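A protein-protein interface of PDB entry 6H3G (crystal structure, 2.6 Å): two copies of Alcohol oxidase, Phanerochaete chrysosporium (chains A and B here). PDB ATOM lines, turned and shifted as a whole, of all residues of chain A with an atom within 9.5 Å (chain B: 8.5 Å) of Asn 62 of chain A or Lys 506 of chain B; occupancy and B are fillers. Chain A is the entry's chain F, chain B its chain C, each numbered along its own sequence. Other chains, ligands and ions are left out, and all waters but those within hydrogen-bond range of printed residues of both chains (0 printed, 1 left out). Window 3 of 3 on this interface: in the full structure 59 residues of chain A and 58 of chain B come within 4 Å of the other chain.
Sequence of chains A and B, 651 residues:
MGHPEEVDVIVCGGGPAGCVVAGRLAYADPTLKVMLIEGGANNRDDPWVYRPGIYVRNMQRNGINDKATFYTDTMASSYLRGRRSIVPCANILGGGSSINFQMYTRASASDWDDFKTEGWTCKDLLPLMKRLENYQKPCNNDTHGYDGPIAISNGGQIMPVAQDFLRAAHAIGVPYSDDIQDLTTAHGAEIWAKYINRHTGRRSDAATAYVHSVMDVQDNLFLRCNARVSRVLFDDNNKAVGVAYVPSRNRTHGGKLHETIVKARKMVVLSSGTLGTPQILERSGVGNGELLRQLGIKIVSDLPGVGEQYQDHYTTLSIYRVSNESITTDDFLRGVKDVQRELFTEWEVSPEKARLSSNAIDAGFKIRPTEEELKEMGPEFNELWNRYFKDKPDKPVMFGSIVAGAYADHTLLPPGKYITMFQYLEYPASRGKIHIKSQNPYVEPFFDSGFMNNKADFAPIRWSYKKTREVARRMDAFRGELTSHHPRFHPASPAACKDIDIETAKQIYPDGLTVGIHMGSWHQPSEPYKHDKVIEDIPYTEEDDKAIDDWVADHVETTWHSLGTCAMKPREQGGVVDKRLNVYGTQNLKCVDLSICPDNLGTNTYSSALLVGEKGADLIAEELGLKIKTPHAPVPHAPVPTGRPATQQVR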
ATOM      1  N   VAL A  56       3.826  15.438 -29.533  1.00  0.00           N
ATOM      2  CA  VAL A  56       4.711  14.861 -28.513  1.00  0.00           C
ATOM      3  C   VAL A  56       3.979  13.768 -27.719  1.00  0.00           C
ATOM      4  O   VAL A  56       4.576  12.722 -27.427  1.00  0.00           O
ATOM      5  CB  VAL A  56       5.289  15.955 -27.594  1.00  0.00           C
ATOM      6  CG1 VAL A  56       5.931  15.375 -26.348  1.00  0.00           C
ATOM      7  CG2 VAL A  56       6.275  16.840 -28.338  1.00  0.00           C
ATOM      8  N   ARG A  57       2.693  13.996 -27.413  1.00  0.00           N
ATOM      9  CA  ARG A  57       1.906  13.157 -26.475  1.00  0.00           C
ATOM     10  C   ARG A  57       1.813  11.687 -26.899  1.00  0.00           C
ATOM     11  O   ARG A  57       1.558  10.845 -26.040  1.00  0.00           O
ATOM     12  CB  ARG A  57       0.464  13.652 -26.295  1.00  0.00           C
ATOM     13  CG  ARG A  57      -0.195  14.188 -27.557  1.00  0.00           C
ATOM     14  CD  ARG A  57      -1.700  14.013 -27.619  1.00  0.00           C
ATOM     15  NE  ARG A  57      -2.367  14.149 -26.335  1.00  0.00           N
ATOM     16  CZ  ARG A  57      -3.544  13.612 -26.061  1.00  0.00           C
ATOM     17  NH1 ARG A  57      -4.238  13.029 -27.023  1.00  0.00           N
ATOM     18  NH2 ARG A  57      -4.013  13.636 -24.828  1.00  0.00           N
ATOM     19  N   ASN A  58       1.975  11.379 -28.192  1.00  0.00           N
ATOM     20  CA  ASN A  58       1.635  10.036 -28.717  1.00  0.00           C
ATOM     21  C   ASN A  58       2.640   8.972 -28.241  1.00  0.00           C
ATOM     22  O   ASN A  58       2.382   7.778 -28.390  1.00  0.00           O
ATOM     23  CB  ASN A  58       1.480  10.052 -30.237  1.00  0.00           C
ATOM     24  CG  ASN A  58       0.409  11.017 -30.702  1.00  0.00           C
ATOM     25  OD1 ASN A  58      -0.724  10.968 -30.220  1.00  0.00           O
ATOM     26  ND2 ASN A  58       0.762  11.896 -31.632  1.00  0.00           N
ATOM     27  N   MET A  59       3.751   9.396 -27.625  1.00  0.00           N
ATOM     28  CA  MET A  59       4.743   8.471 -27.089  1.00  0.00           C
ATOM     29  C   MET A  59       4.619   8.314 -25.561  1.00  0.00           C
ATOM     30  O   MET A  59       5.409   7.561 -24.966  1.00  0.00           O
ATOM     31  CB  MET A  59       6.152   8.941 -27.465  1.00  0.00           C
ATOM     32  CG  MET A  59       6.546   8.539 -28.873  1.00  0.00           C
ATOM     33  SD  MET A  59       6.393   6.742 -29.111  1.00  0.00           S
ATOM     34  CE  MET A  59       5.043   6.613 -30.283  1.00  0.00           C
ATOM     35  N   GLN A  60       3.626   8.978 -24.938  1.00  0.00           N
ATOM     36  CA  GLN A  60       3.323   8.837 -23.487  1.00  0.00           C
ATOM     37  C   GLN A  60       2.860   7.400 -23.201  1.00  0.00           C
ATOM     38  O   GLN A  60       1.922   6.908 -23.844  1.00  0.00           O
ATOM     39  CB  GLN A  60       2.235   9.809 -22.997  1.00  0.00           C
ATOM     40  CG  GLN A  60       2.700  11.250 -22.786  1.00  0.00           C
ATOM     41  CD  GLN A  60       1.590  12.193 -22.372  1.00  0.00           C
ATOM     42  OE1 GLN A  60       0.560  12.310 -23.029  1.00  0.00           O
ATOM     43  NE2 GLN A  60       1.805  12.915 -21.285  1.00  0.00           N
ATOM     44  N   ARG A  61       3.557   6.746 -22.265  1.00  0.00           N
ATOM     45  CA  ARG A  61       3.174   5.466 -21.690  1.00  0.00           C
ATOM     46  C   ARG A  61       2.506   5.747 -20.341  1.00  0.00           C
ATOM     47  O   ARG A  61       3.136   5.615 -19.298  1.00  0.00           O
ATOM     48  CB  ARG A  61       4.413   4.578 -21.522  1.00  0.00           C
ATOM     49  CG  ARG A  61       5.123   4.239 -22.825  1.00  0.00           C
ATOM     50  CD  ARG A  61       6.632   4.134 -22.675  1.00  0.00           C
ATOM     51  NE  ARG A  61       7.058   3.207 -21.631  1.00  0.00           N
ATOM     52  CZ  ARG A  61       7.700   3.559 -20.520  1.00  0.00           C
ATOM     53  NH1 ARG A  61       7.954   4.832 -20.268  1.00  0.00           N
ATOM     54  NH2 ARG A  61       8.100   2.633 -19.672  1.00  0.00           N
ATOM     55  N   ASN A  62       1.240   6.170 -20.383  1.00  0.00           N
ATOM     56  CA  ASN A  62       0.568   6.755 -19.191  1.00  0.00           C
ATOM     57  C   ASN A  62      -0.784   6.103 -18.866  1.00  0.00           C
ATOM     58  O   ASN A  62      -1.540   6.666 -18.109  1.00  0.00           O
ATOM     59  CB  ASN A  62       0.354   8.264 -19.358  1.00  0.00           C
ATOM     60  CG  ASN A  62      -0.548   8.623 -20.522  1.00  0.00           C
ATOM     61  OD1 ASN A  62      -1.210   7.765 -21.097  1.00  0.00           O
ATOM     62  ND2 ASN A  62      -0.575   9.893 -20.886  1.00  0.00           N
ATOM     63  N   GLY A  63      -1.092   4.938 -19.437  1.00  0.00           N
ATOM     64  CA  GLY A  63      -2.339   4.245 -19.128  1.00  0.00           C
ATOM     65  C   GLY A  63      -3.538   4.760 -19.921  1.00  0.00           C
ATOM     66  O   GLY A  63      -4.545   4.058 -20.006  1.00  0.00           O
ATOM     67  N   ILE A  64      -3.433   5.969 -20.498  1.00  0.00           N
ATOM     68  CA  ILE A  64      -4.514   6.622 -21.264  1.00  0.00           C
ATOM     69  C   ILE A  64      -4.243   6.459 -22.766  1.00  0.00           C
ATOM     70  O   ILE A  64      -5.094   5.924 -23.474  1.00  0.00           O
ATOM     71  CB  ILE A  64      -4.666   8.113 -20.887  1.00  0.00           C
ATOM     72  CG1 ILE A  64      -4.880   8.316 -19.383  1.00  0.00           C
ATOM     73  CG2 ILE A  64      -5.780   8.771 -21.695  1.00  0.00           C
ATOM     74  CD1 ILE A  64      -4.595   9.727 -18.903  1.00  0.00           C
ATOM     75  N   ASN A  65      -3.074   6.939 -23.226  1.00  0.00           N
ATOM     76  CA  ASN A  65      -2.661   6.960 -24.659  1.00  0.00           C
ATOM     77  C   ASN A  65      -2.793   5.564 -25.276  1.00  0.00           C
ATOM     78  O   ASN A  65      -2.298   4.616 -24.702  1.00  0.00           O
ATOM     79  CB  ASN A  65      -1.208   7.409 -24.836  1.00  0.00           C
ATOM     80  CG  ASN A  65      -0.734   7.291 -26.271  1.00  0.00           C
ATOM     81  OD1 ASN A  65      -1.214   8.012 -27.145  1.00  0.00           O
ATOM     82  ND2 ASN A  65       0.192   6.379 -26.527  1.00  0.00           N
ATOM     83  N   ASP A  66      -3.438   5.445 -26.445  1.00  0.00           N
ATOM     84  CA  ASP A  66      -3.553   4.123 -27.098  1.00  0.00           C
ATOM     85  C   ASP A  66      -3.222   4.188 -28.597  1.00  0.00           C
ATOM     86  O   ASP A  66      -3.567   3.262 -29.322  1.00  0.00           O
ATOM     87  CB  ASP A  66      -4.923   3.478 -26.852  1.00  0.00           C
ATOM     88  CG  ASP A  66      -6.042   4.036 -27.702  1.00  0.00           C
ATOM     89  OD1 ASP A  66      -5.865   5.163 -28.211  1.00  0.00           O
ATOM     90  OD2 ASP A  66      -7.074   3.337 -27.855  1.00  0.00           O
ATOM     91  N   LYS A  67      -2.491   5.223 -29.039  1.00  0.00           N
ATOM     92  CA  LYS A  67      -2.101   5.366 -30.452  1.00  0.00           C
ATOM     93  C   LYS A  67      -0.713   4.758 -30.713  1.00  0.00           C
ATOM     94  O   LYS A  67      -0.030   5.163 -31.660  1.00  0.00           O
ATOM     95  CB  LYS A  67      -2.061   6.838 -30.871  1.00  0.00           C
ATOM     96  CG  LYS A  67      -3.344   7.623 -30.664  1.00  0.00           C
ATOM     97  CD  LYS A  67      -3.241   9.036 -31.190  1.00  0.00           C
ATOM     98  CE  LYS A  67      -3.937  10.039 -30.303  1.00  0.00           C
ATOM     99  NZ  LYS A  67      -5.396   9.785 -30.274  1.00  0.00           N
ATOM    100  N   ALA A  68      -0.292   3.787 -29.894  1.00  0.00           N
ATOM    101  CA  ALA A  68       1.011   3.163 -30.056  1.00  0.00           C
ATOM    102  C   ALA A  68       1.039   1.803 -29.350  1.00  0.00           C
ATOM    103  O   ALA A  68       0.486   1.653 -28.264  1.00  0.00           O
ATOM    104  CB  ALA A  68       2.070   4.086 -29.510  1.00  0.00           C
ATOM    105  N   PHE A  70       3.800  -0.848 -27.738  1.00  0.00           N
ATOM    106  CA  PHE A  70       5.138  -0.819 -27.228  1.00  0.00           C
ATOM    107  C   PHE A  70       5.683  -2.246 -27.276  1.00  0.00           C
ATOM    108  O   PHE A  70       5.096  -3.150 -26.692  1.00  0.00           O
ATOM    109  CB  PHE A  70       5.130  -0.179 -25.838  1.00  0.00           C
ATOM    110  CG  PHE A  70       4.673   1.259 -25.849  1.00  0.00           C
ATOM    111  CD1 PHE A  70       5.545   2.274 -26.207  1.00  0.00           C
ATOM    112  CD2 PHE A  70       3.363   1.597 -25.545  1.00  0.00           C
ATOM    113  CE1 PHE A  70       5.122   3.595 -26.243  1.00  0.00           C
ATOM    114  CE2 PHE A  70       2.942   2.919 -25.585  1.00  0.00           C
ATOM    115  CZ  PHE A  70       3.821   3.915 -25.934  1.00  0.00           C
ATOM    116  N   ARG A 334       4.453  21.028 -20.489  1.00  0.00           N
ATOM    117  CA  ARG A 334       4.225  20.901 -19.050  1.00  0.00           C
ATOM    118  C   ARG A 334       2.713  20.847 -18.776  1.00  0.00           C
ATOM    119  O   ARG A 334       2.264  20.156 -17.863  1.00  0.00           O
ATOM    120  CB  ARG A 334       4.923  22.030 -18.277  1.00  0.00           C
ATOM    121  CG  ARG A 334       6.389  21.753 -17.966  1.00  0.00           C
ATOM    122  CD  ARG A 334       7.132  22.945 -17.393  1.00  0.00           C
ATOM    123  NE  ARG A 334       8.545  22.656 -17.163  1.00  0.00           N
ATOM    124  CZ  ARG A 334       9.569  23.399 -17.590  1.00  0.00           C
ATOM    125  NH1 ARG A 334       9.359  24.528 -18.247  1.00  0.00           N
ATOM    126  NH2 ARG A 334      10.808  23.011 -17.350  1.00  0.00           N
ATOM    127  N   ASP A 409      10.820  13.603 -20.542  1.00  0.00           N
ATOM    128  CA  ASP A 409       9.869  13.675 -19.439  1.00  0.00           C
ATOM    129  C   ASP A 409      10.202  14.880 -18.545  1.00  0.00           C
ATOM    130  O   ASP A 409      11.220  14.872 -17.867  1.00  0.00           O
ATOM    131  CB  ASP A 409       9.902  12.357 -18.664  1.00  0.00           C
ATOM    132  CG  ASP A 409       8.685  12.124 -17.797  1.00  0.00           C
ATOM    133  OD1 ASP A 409       8.003  13.115 -17.496  1.00  0.00           O
ATOM    134  OD2 ASP A 409       8.424  10.945 -17.455  1.00  0.00           O
ATOM    135  N   HIS A 410       9.331  15.902 -18.546  1.00  0.00           N
ATOM    136  CA  HIS A 410       9.562  17.193 -17.842  1.00  0.00           C
ATOM    137  C   HIS A 410       9.484  17.005 -16.321  1.00  0.00           C
ATOM    138  O   HIS A 410      10.037  17.822 -15.544  1.00  0.00           O
ATOM    139  CB  HIS A 410       8.587  18.269 -18.336  1.00  0.00           C
ATOM    140  CG  HIS A 410       8.945  18.833 -19.671  1.00  0.00           C
ATOM    141  ND1 HIS A 410       8.805  18.108 -20.842  1.00  0.00           N
ATOM    142  CD2 HIS A 410       9.438  20.040 -20.027  1.00  0.00           C
ATOM    143  CE1 HIS A 410       9.203  18.846 -21.861  1.00  0.00           C
ATOM    144  NE2 HIS A 410       9.594  20.036 -21.392  1.00  0.00           N
ATOM    145  N   THR A 411       8.785  15.931 -15.934  1.00  0.00           N
ATOM    146  CA  THR A 411       8.804  15.307 -14.614  1.00  0.00           C
ATOM    147  C   THR A 411      10.246  15.010 -14.148  1.00  0.00           C
ATOM    148  O   THR A 411      10.482  14.939 -12.959  1.00  0.00           O
ATOM    149  CB  THR A 411       7.876  14.081 -14.652  1.00  0.00           C
ATOM    150  OG1 THR A 411       6.752  14.301 -13.797  1.00  0.00           O
ATOM    151  CG2 THR A 411       8.558  12.781 -14.291  1.00  0.00           C
ATOM    152  N   ASN B 324       2.972  13.337  -3.482  1.00  0.00           N
ATOM    153  CA  ASN B 324       2.568  14.735  -3.663  1.00  0.00           C
ATOM    154  C   ASN B 324       1.609  15.182  -2.557  1.00  0.00           C
ATOM    155  O   ASN B 324       1.408  16.376  -2.393  1.00  0.00           O
ATOM    156  CB  ASN B 324       1.932  14.984  -5.033  1.00  0.00           C
ATOM    157  CG  ASN B 324       2.945  15.009  -6.156  1.00  0.00           C
ATOM    158  OD1 ASN B 324       3.753  15.936  -6.245  1.00  0.00           O
ATOM    159  ND2 ASN B 324       2.900  13.994  -7.005  1.00  0.00           N
ATOM    160  N   ILE B 500      11.249   8.633  -9.834  1.00  0.00           N
ATOM    161  CA  ILE B 500       9.817   8.732  -9.605  1.00  0.00           C
ATOM    162  C   ILE B 500       9.051   7.656 -10.390  1.00  0.00           C
ATOM    163  O   ILE B 500       9.443   7.255 -11.503  1.00  0.00           O
ATOM    164  CB  ILE B 500       9.315  10.147  -9.944  1.00  0.00           C
ATOM    165  CG1 ILE B 500       7.887  10.359  -9.434  1.00  0.00           C
ATOM    166  CG2 ILE B 500       9.445  10.435 -11.433  1.00  0.00           C
ATOM    167  CD1 ILE B 500       7.464  11.804  -9.383  1.00  0.00           C
ATOM    168  N   ASP B 501       7.950   7.200  -9.774  1.00  0.00           N
ATOM    169  CA  ASP B 501       7.047   6.201 -10.321  1.00  0.00           C
ATOM    170  C   ASP B 501       5.959   6.917 -11.125  1.00  0.00           C
ATOM    171  O   ASP B 501       5.698   8.108 -10.918  1.00  0.00           O
ATOM    172  CB  ASP B 501       6.410   5.360  -9.219  1.00  0.00           C
ATOM    173  CG  ASP B 501       5.401   6.136  -8.401  1.00  0.00           C
ATOM    174  OD1 ASP B 501       5.823   7.036  -7.658  1.00  0.00           O
ATOM    175  OD2 ASP B 501       4.205   5.851  -8.535  1.00  0.00           O
ATOM    176  N   ILE B 502       5.320   6.181 -12.038  1.00  0.00           N
ATOM    177  CA  ILE B 502       4.541   6.826 -13.098  1.00  0.00           C
ATOM    178  C   ILE B 502       3.294   7.500 -12.498  1.00  0.00           C
ATOM    179  O   ILE B 502       2.942   8.605 -12.909  1.00  0.00           O
ATOM    180  CB  ILE B 502       4.231   5.854 -14.263  1.00  0.00           C
ATOM    181  CG1 ILE B 502       3.486   6.559 -15.401  1.00  0.00           C
ATOM    182  CG2 ILE B 502       3.484   4.606 -13.792  1.00  0.00           C
ATOM    183  CD1 ILE B 502       4.225   7.733 -16.011  1.00  0.00           C
ATOM    184  N   GLU B 503       2.662   6.852 -11.510  1.00  0.00           N
ATOM    185  CA  GLU B 503       1.463   7.384 -10.849  1.00  0.00           C
ATOM    186  C   GLU B 503       1.755   8.766 -10.252  1.00  0.00           C
ATOM    187  O   GLU B 503       0.928   9.676 -10.356  1.00  0.00           O
ATOM    188  CB  GLU B 503       0.981   6.438  -9.748  1.00  0.00           C
ATOM    189  CG  GLU B 503       0.423   5.119 -10.258  1.00  0.00           C
ATOM    190  CD  GLU B 503      -0.945   5.215 -10.921  1.00  0.00           C
ATOM    191  OE1 GLU B 503      -1.829   4.403 -10.563  1.00  0.00           O
ATOM    192  OE2 GLU B 503      -1.134   6.100 -11.796  1.00  0.00           O
ATOM    193  N   THR B 504       2.936   8.905  -9.636  1.00  0.00           N
ATOM    194  CA  THR B 504       3.315  10.126  -8.921  1.00  0.00           C
ATOM    195  C   THR B 504       3.629  11.230  -9.933  1.00  0.00           C
ATOM    196  O   THR B 504       3.247  12.373  -9.717  1.00  0.00           O
ATOM    197  CB  THR B 504       4.483   9.886  -7.948  1.00  0.00           C
ATOM    198  OG1 THR B 504       4.139   8.816  -7.069  1.00  0.00           O
ATOM    199  CG2 THR B 504       4.823  11.094  -7.106  1.00  0.00           C
ATOM    200  N   ALA B 505       4.319  10.872 -11.022  1.00  0.00           N
ATOM    201  CA  ALA B 505       4.691  11.823 -12.090  1.00  0.00           C
ATOM    202  C   ALA B 505       3.445  12.473 -12.727  1.00  0.00           C
ATOM    203  O   ALA B 505       3.390  13.688 -12.900  1.00  0.00           O
ATOM    204  CB  ALA B 505       5.536  11.121 -13.122  1.00  0.00           C
ATOM    205  N   LYS B 506       2.431  11.666 -13.050  1.00  0.00           N
ATOM    206  CA  LYS B 506       1.213  12.159 -13.722  1.00  0.00           C
ATOM    207  C   LYS B 506       0.492  13.207 -12.865  1.00  0.00           C
ATOM    208  O   LYS B 506      -0.139  14.112 -13.418  1.00  0.00           O
ATOM    209  CB  LYS B 506       0.244  11.015 -14.042  1.00  0.00           C
ATOM    210  CG  LYS B 506       0.732  10.036 -15.098  1.00  0.00           C
ATOM    211  CD  LYS B 506       0.059   8.690 -15.016  1.00  0.00           C
ATOM    212  CE  LYS B 506      -1.328   8.680 -15.617  1.00  0.00           C
ATOM    213  NZ  LYS B 506      -1.975   7.364 -15.425  1.00  0.00           N
ATOM    214  N   GLN B 507       0.559  13.074 -11.533  1.00  0.00           N
ATOM    215  CA  GLN B 507      -0.096  14.039 -10.632  1.00  0.00           C
ATOM    216  C   GLN B 507       0.624  15.392 -10.675  1.00  0.00           C
ATOM    217  O   GLN B 507       0.011  16.418 -10.412  1.00  0.00           O
ATOM    218  CB  GLN B 507      -0.145  13.525  -9.196  1.00  0.00           C
ATOM    219  CG  GLN B 507      -1.083  12.341  -9.009  1.00  0.00           C
ATOM    220  CD  GLN B 507      -0.947  11.714  -7.640  1.00  0.00           C
ATOM    221  OE1 GLN B 507      -0.437  12.330  -6.706  1.00  0.00           O
ATOM    222  NE2 GLN B 507      -1.402  10.477  -7.511  1.00  0.00           N
ATOM    223  N   ILE B 508       1.919  15.400 -11.001  1.00  0.00           N
ATOM    224  CA  ILE B 508       2.653  16.650 -11.063  1.00  0.00           C
ATOM    225  C   ILE B 508       2.160  17.456 -12.266  1.00  0.00           C
ATOM    226  O   ILE B 508       1.817  18.629 -12.129  1.00  0.00           O
ATOM    227  CB  ILE B 508       4.172  16.411 -11.117  1.00  0.00           C
ATOM    228  CG1 ILE B 508       4.681  15.836  -9.796  1.00  0.00           C
ATOM    229  CG2 ILE B 508       4.906  17.693 -11.488  1.00  0.00           C
ATOM    230  CD1 ILE B 508       6.029  15.167  -9.893  1.00  0.00           C
ATOM    231  N   TYR B 509       2.136  16.809 -13.436  1.00  0.00           N
ATOM    232  CA  TYR B 509       1.759  17.446 -14.679  1.00  0.00           C
ATOM    233  C   TYR B 509       0.619  16.674 -15.336  1.00  0.00           C
ATOM    234  O   TYR B 509       0.842  15.970 -16.319  1.00  0.00           O
ATOM    235  CB  TYR B 509       2.952  17.483 -15.632  1.00  0.00           C
ATOM    236  CG  TYR B 509       4.069  18.428 -15.272  1.00  0.00           C
ATOM    237  CD1 TYR B 509       3.817  19.702 -14.789  1.00  0.00           C
ATOM    238  CD2 TYR B 509       5.390  18.063 -15.495  1.00  0.00           C
ATOM    239  CE1 TYR B 509       4.854  20.572 -14.495  1.00  0.00           C
ATOM    240  CE2 TYR B 509       6.439  18.923 -15.212  1.00  0.00           C
ATOM    241  CZ  TYR B 509       6.165  20.180 -14.711  1.00  0.00           C
ATOM    242  OH  TYR B 509       7.196  21.016 -14.427  1.00  0.00           O
ATOM    243  N   PRO B 510      -0.631  16.774 -14.832  1.00  0.00           N
ATOM    244  CA  PRO B 510      -1.736  15.980 -15.381  1.00  0.00           C
ATOM    245  C   PRO B 510      -2.282  16.404 -16.763  1.00  0.00           C
ATOM    246  O   PRO B 510      -3.144  15.708 -17.299  1.00  0.00           O
ATOM    247  CB  PRO B 510      -2.814  16.109 -14.291  1.00  0.00           C
ATOM    248  CG  PRO B 510      -2.540  17.451 -13.651  1.00  0.00           C
ATOM    249  CD  PRO B 510      -1.035  17.600 -13.685  1.00  0.00           C
ATOM    250  N   ASP B 511      -1.810  17.527 -17.322  1.00  0.00           N
ATOM    251  CA  ASP B 511      -2.144  17.916 -18.698  1.00  0.00           C
ATOM    252  C   ASP B 511      -0.865  17.936 -19.551  1.00  0.00           C
ATOM    253  O   ASP B 511      -0.911  18.280 -20.742  1.00  0.00           O
ATOM    254  CB  ASP B 511      -2.881  19.259 -18.756  1.00  0.00           C
ATOM    255  CG  ASP B 511      -4.203  19.289 -18.003  1.00  0.00           C
ATOM    256  OD1 ASP B 511      -4.858  18.232 -17.923  1.00  0.00           O
ATOM    257  OD2 ASP B 511      -4.568  20.372 -17.495  1.00  0.00           O
ATOM    258  N   GLY B 512       0.262  17.533 -18.948  1.00  0.00           N
ATOM    259  CA  GLY B 512       1.559  17.505 -19.608  1.00  0.00           C
ATOM    260  C   GLY B 512       1.595  16.458 -20.705  1.00  0.00           C
ATOM    261  O   GLY B 512       0.966  15.398 -20.592  1.00  0.00           O
ATOM    262  N   LEU B 513       2.328  16.768 -21.779  1.00  0.00           N
ATOM    263  CA  LEU B 513       2.334  15.955 -22.994  1.00  0.00           C
ATOM    264  C   LEU B 513       3.474  14.934 -22.903  1.00  0.00           C
ATOM    265  O   LEU B 513       3.651  14.116 -23.784  1.00  0.00           O
ATOM    266  CB  LEU B 513       2.552  16.847 -24.223  1.00  0.00           C
ATOM    267  CG  LEU B 513       1.459  17.836 -24.644  1.00  0.00           C
ATOM    268  CD1 LEU B 513       0.713  17.326 -25.864  1.00  0.00           C
ATOM    269  CD2 LEU B 513       0.484  18.189 -23.537  1.00  0.00           C
ATOM    270  N   THR B 514       4.240  14.987 -21.815  1.00  0.00           N
ATOM    271  CA  THR B 514       5.604  14.468 -21.810  1.00  0.00           C
ATOM    272  C   THR B 514       5.833  13.405 -20.715  1.00  0.00           C
ATOM    273  O   THR B 514       6.891  12.779 -20.694  1.00  0.00           O
ATOM    274  CB  THR B 514       6.561  15.659 -21.699  1.00  0.00           C
ATOM    275  OG1 THR B 514       7.888  15.152 -21.797  1.00  0.00           O
ATOM    276  CG2 THR B 514       6.360  16.442 -20.418  1.00  0.00           C
ATOM    277  N   VAL B 515       4.843  13.183 -19.838  1.00  0.00           N
ATOM    278  CA  VAL B 515       4.951  12.275 -18.693  1.00  0.00           C
ATOM    279  C   VAL B 515       4.835  10.833 -19.184  1.00  0.00           C
ATOM    280  O   VAL B 515       3.806  10.442 -19.685  1.00  0.00           O
ATOM    281  CB  VAL B 515       3.874  12.587 -17.634  1.00  0.00           C
ATOM    282  CG1 VAL B 515       3.723  11.485 -16.590  1.00  0.00           C
ATOM    283  CG2 VAL B 515       4.142  13.929 -16.963  1.00  0.00           C
ATOM    284  N   GLY B 516       5.901  10.049 -19.009  1.00  0.00           N
ATOM    285  CA  GLY B 516       5.869   8.634 -19.332  1.00  0.00           C
ATOM    286  C   GLY B 516       6.501   8.347 -20.681  1.00  0.00           C
ATOM    287  O   GLY B 516       6.529   7.203 -21.121  1.00  0.00           O
ATOM    288  N   ILE B 517       6.995   9.396 -21.342  1.00  0.00           N
ATOM    289  CA  ILE B 517       7.841   9.239 -22.501  1.00  0.00           C
ATOM    290  C   ILE B 517       9.168   8.671 -22.008  1.00  0.00           C
ATOM    291  O   ILE B 517       9.902   9.363 -21.313  1.00  0.00           O
ATOM    292  CB  ILE B 517       8.034  10.577 -23.241  1.00  0.00           C
ATOM    293  CG1 ILE B 517       6.723  11.046 -23.869  1.00  0.00           C
ATOM    294  CG2 ILE B 517       9.151  10.488 -24.274  1.00  0.00           C
ATOM    295  CD1 ILE B 517       6.826  12.384 -24.557  1.00  0.00           C
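Of the 18 printed residues of chain A, 10 touch a printed residue of chain B. Printed residues of chain B that touch a printed residue of chain A: Ile 500, Ala 505, Lys 506, Tyr 509, Gly 512, Leu 513, Thr 514, Val 515, Gly 516 and Ile 517. Hydrophobic or aromatic side chains of chain B within 4 Å of the printed part of chain A: Ile 500, Ala 505, Tyr 509, Leu 513, Val 515 and Ile 517. Among the printed residues, no Asp or Glu carboxylate lies within 4 Å of a Lys or Arg side-chain nitrogen of the other chain.
OE1 of Gln 60 of chain A lies within hydrogen-bond range of ND2 of Asn 62 of chain A, at 3.4 Å. N of Ile 64 of chain A sits at hydrogen-bond distance from OD1 of Asn 62 of chain A (2.9 Å).
The guanidinium group (NE) of Arg 334 of chain A sits at hydrogen-bond distance from the side-chain hydroxyl (OH) of Tyr 509 of chain B (3.5 Å). The backbone NH (N) of Thr 514 of chain B sits close to the side-chain amide nitrogen (NE2) of Gln 60 of chain A, at 3.2 Å. The backbone carbonyl oxygen (O) of Gly 512 of chain B lies within hydrogen-bond range of the side-chain amide nitrogen (NE2) of Gln 60 of chain A, at 2.7 Å. The side-chain amino group (NZ) of Lys 506 of chain B sits at hydrogen-bond distance from the backbone carbonyl oxygen (O) of Asn 62 of chain A (2.8 Å). O of Leu 513 of chain B lies close to NE2 of Gln 60 of chain A (3.3 Å). N of Val 515 of chain B lies close to NE2 of Gln 60 of chain A (3.4 Å). OD2 of Asp 409 of chain A lies within hydrogen-bond range of N of Gly 516 of chain B, 3.1 Å away. O of Gly 516 of chain B lies within hydrogen-bond range of NH1 of Arg 61 of chain A. The side-chain carboxylate (OD1) of Asp 409 of chain A sits close to the backbone carbonyl oxygen (O) of Thr 514 of chain B (3.4 Å). The backbone NH of Gly 512 of chain B sits close to the backbone carbonyl oxygen of Arg 334 of chain A, 3.5 Å away.
No position is printed for both chains. Of the 22 pairs that touch across the chains among the printed residues, none has its exchanged pair printed and touching as well.
Of the printed residues of chain B, Val 56 of chain A touches Leu 513 and Ile 517. No residue of chain B comes within 4 Å of Gly 63 of chain A. Ala 505 of chain B touches just one residue of chain A: Thr 411 (3.5 Å). No residue of chain A comes within 4 Å of Pro 510 of chain B. Of the printed residues of chain A, Ile 517 of chain B touches Val 56 (3.6 Å), Met 59 (3.8 Å), Gln 60 (3.9 Å) and Asp 409 (3.998 Å). The nearest residue of chain B that does not touch Asn 62 of chain A is Val 515 of chain B (4.1 Å).
Val 56 of chain A touches Ile 517 of chain B (CG1 to CD1, 3.6 Å). CG1 of Ile 517 of chain B touches C of Met 59 of chain A (3.8 Å). Ile 517 of chain B touches Gln 60 of chain A (CG1 to N, 3.9 Å). Val 515 of chain B touches Asp 409 of chain A.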
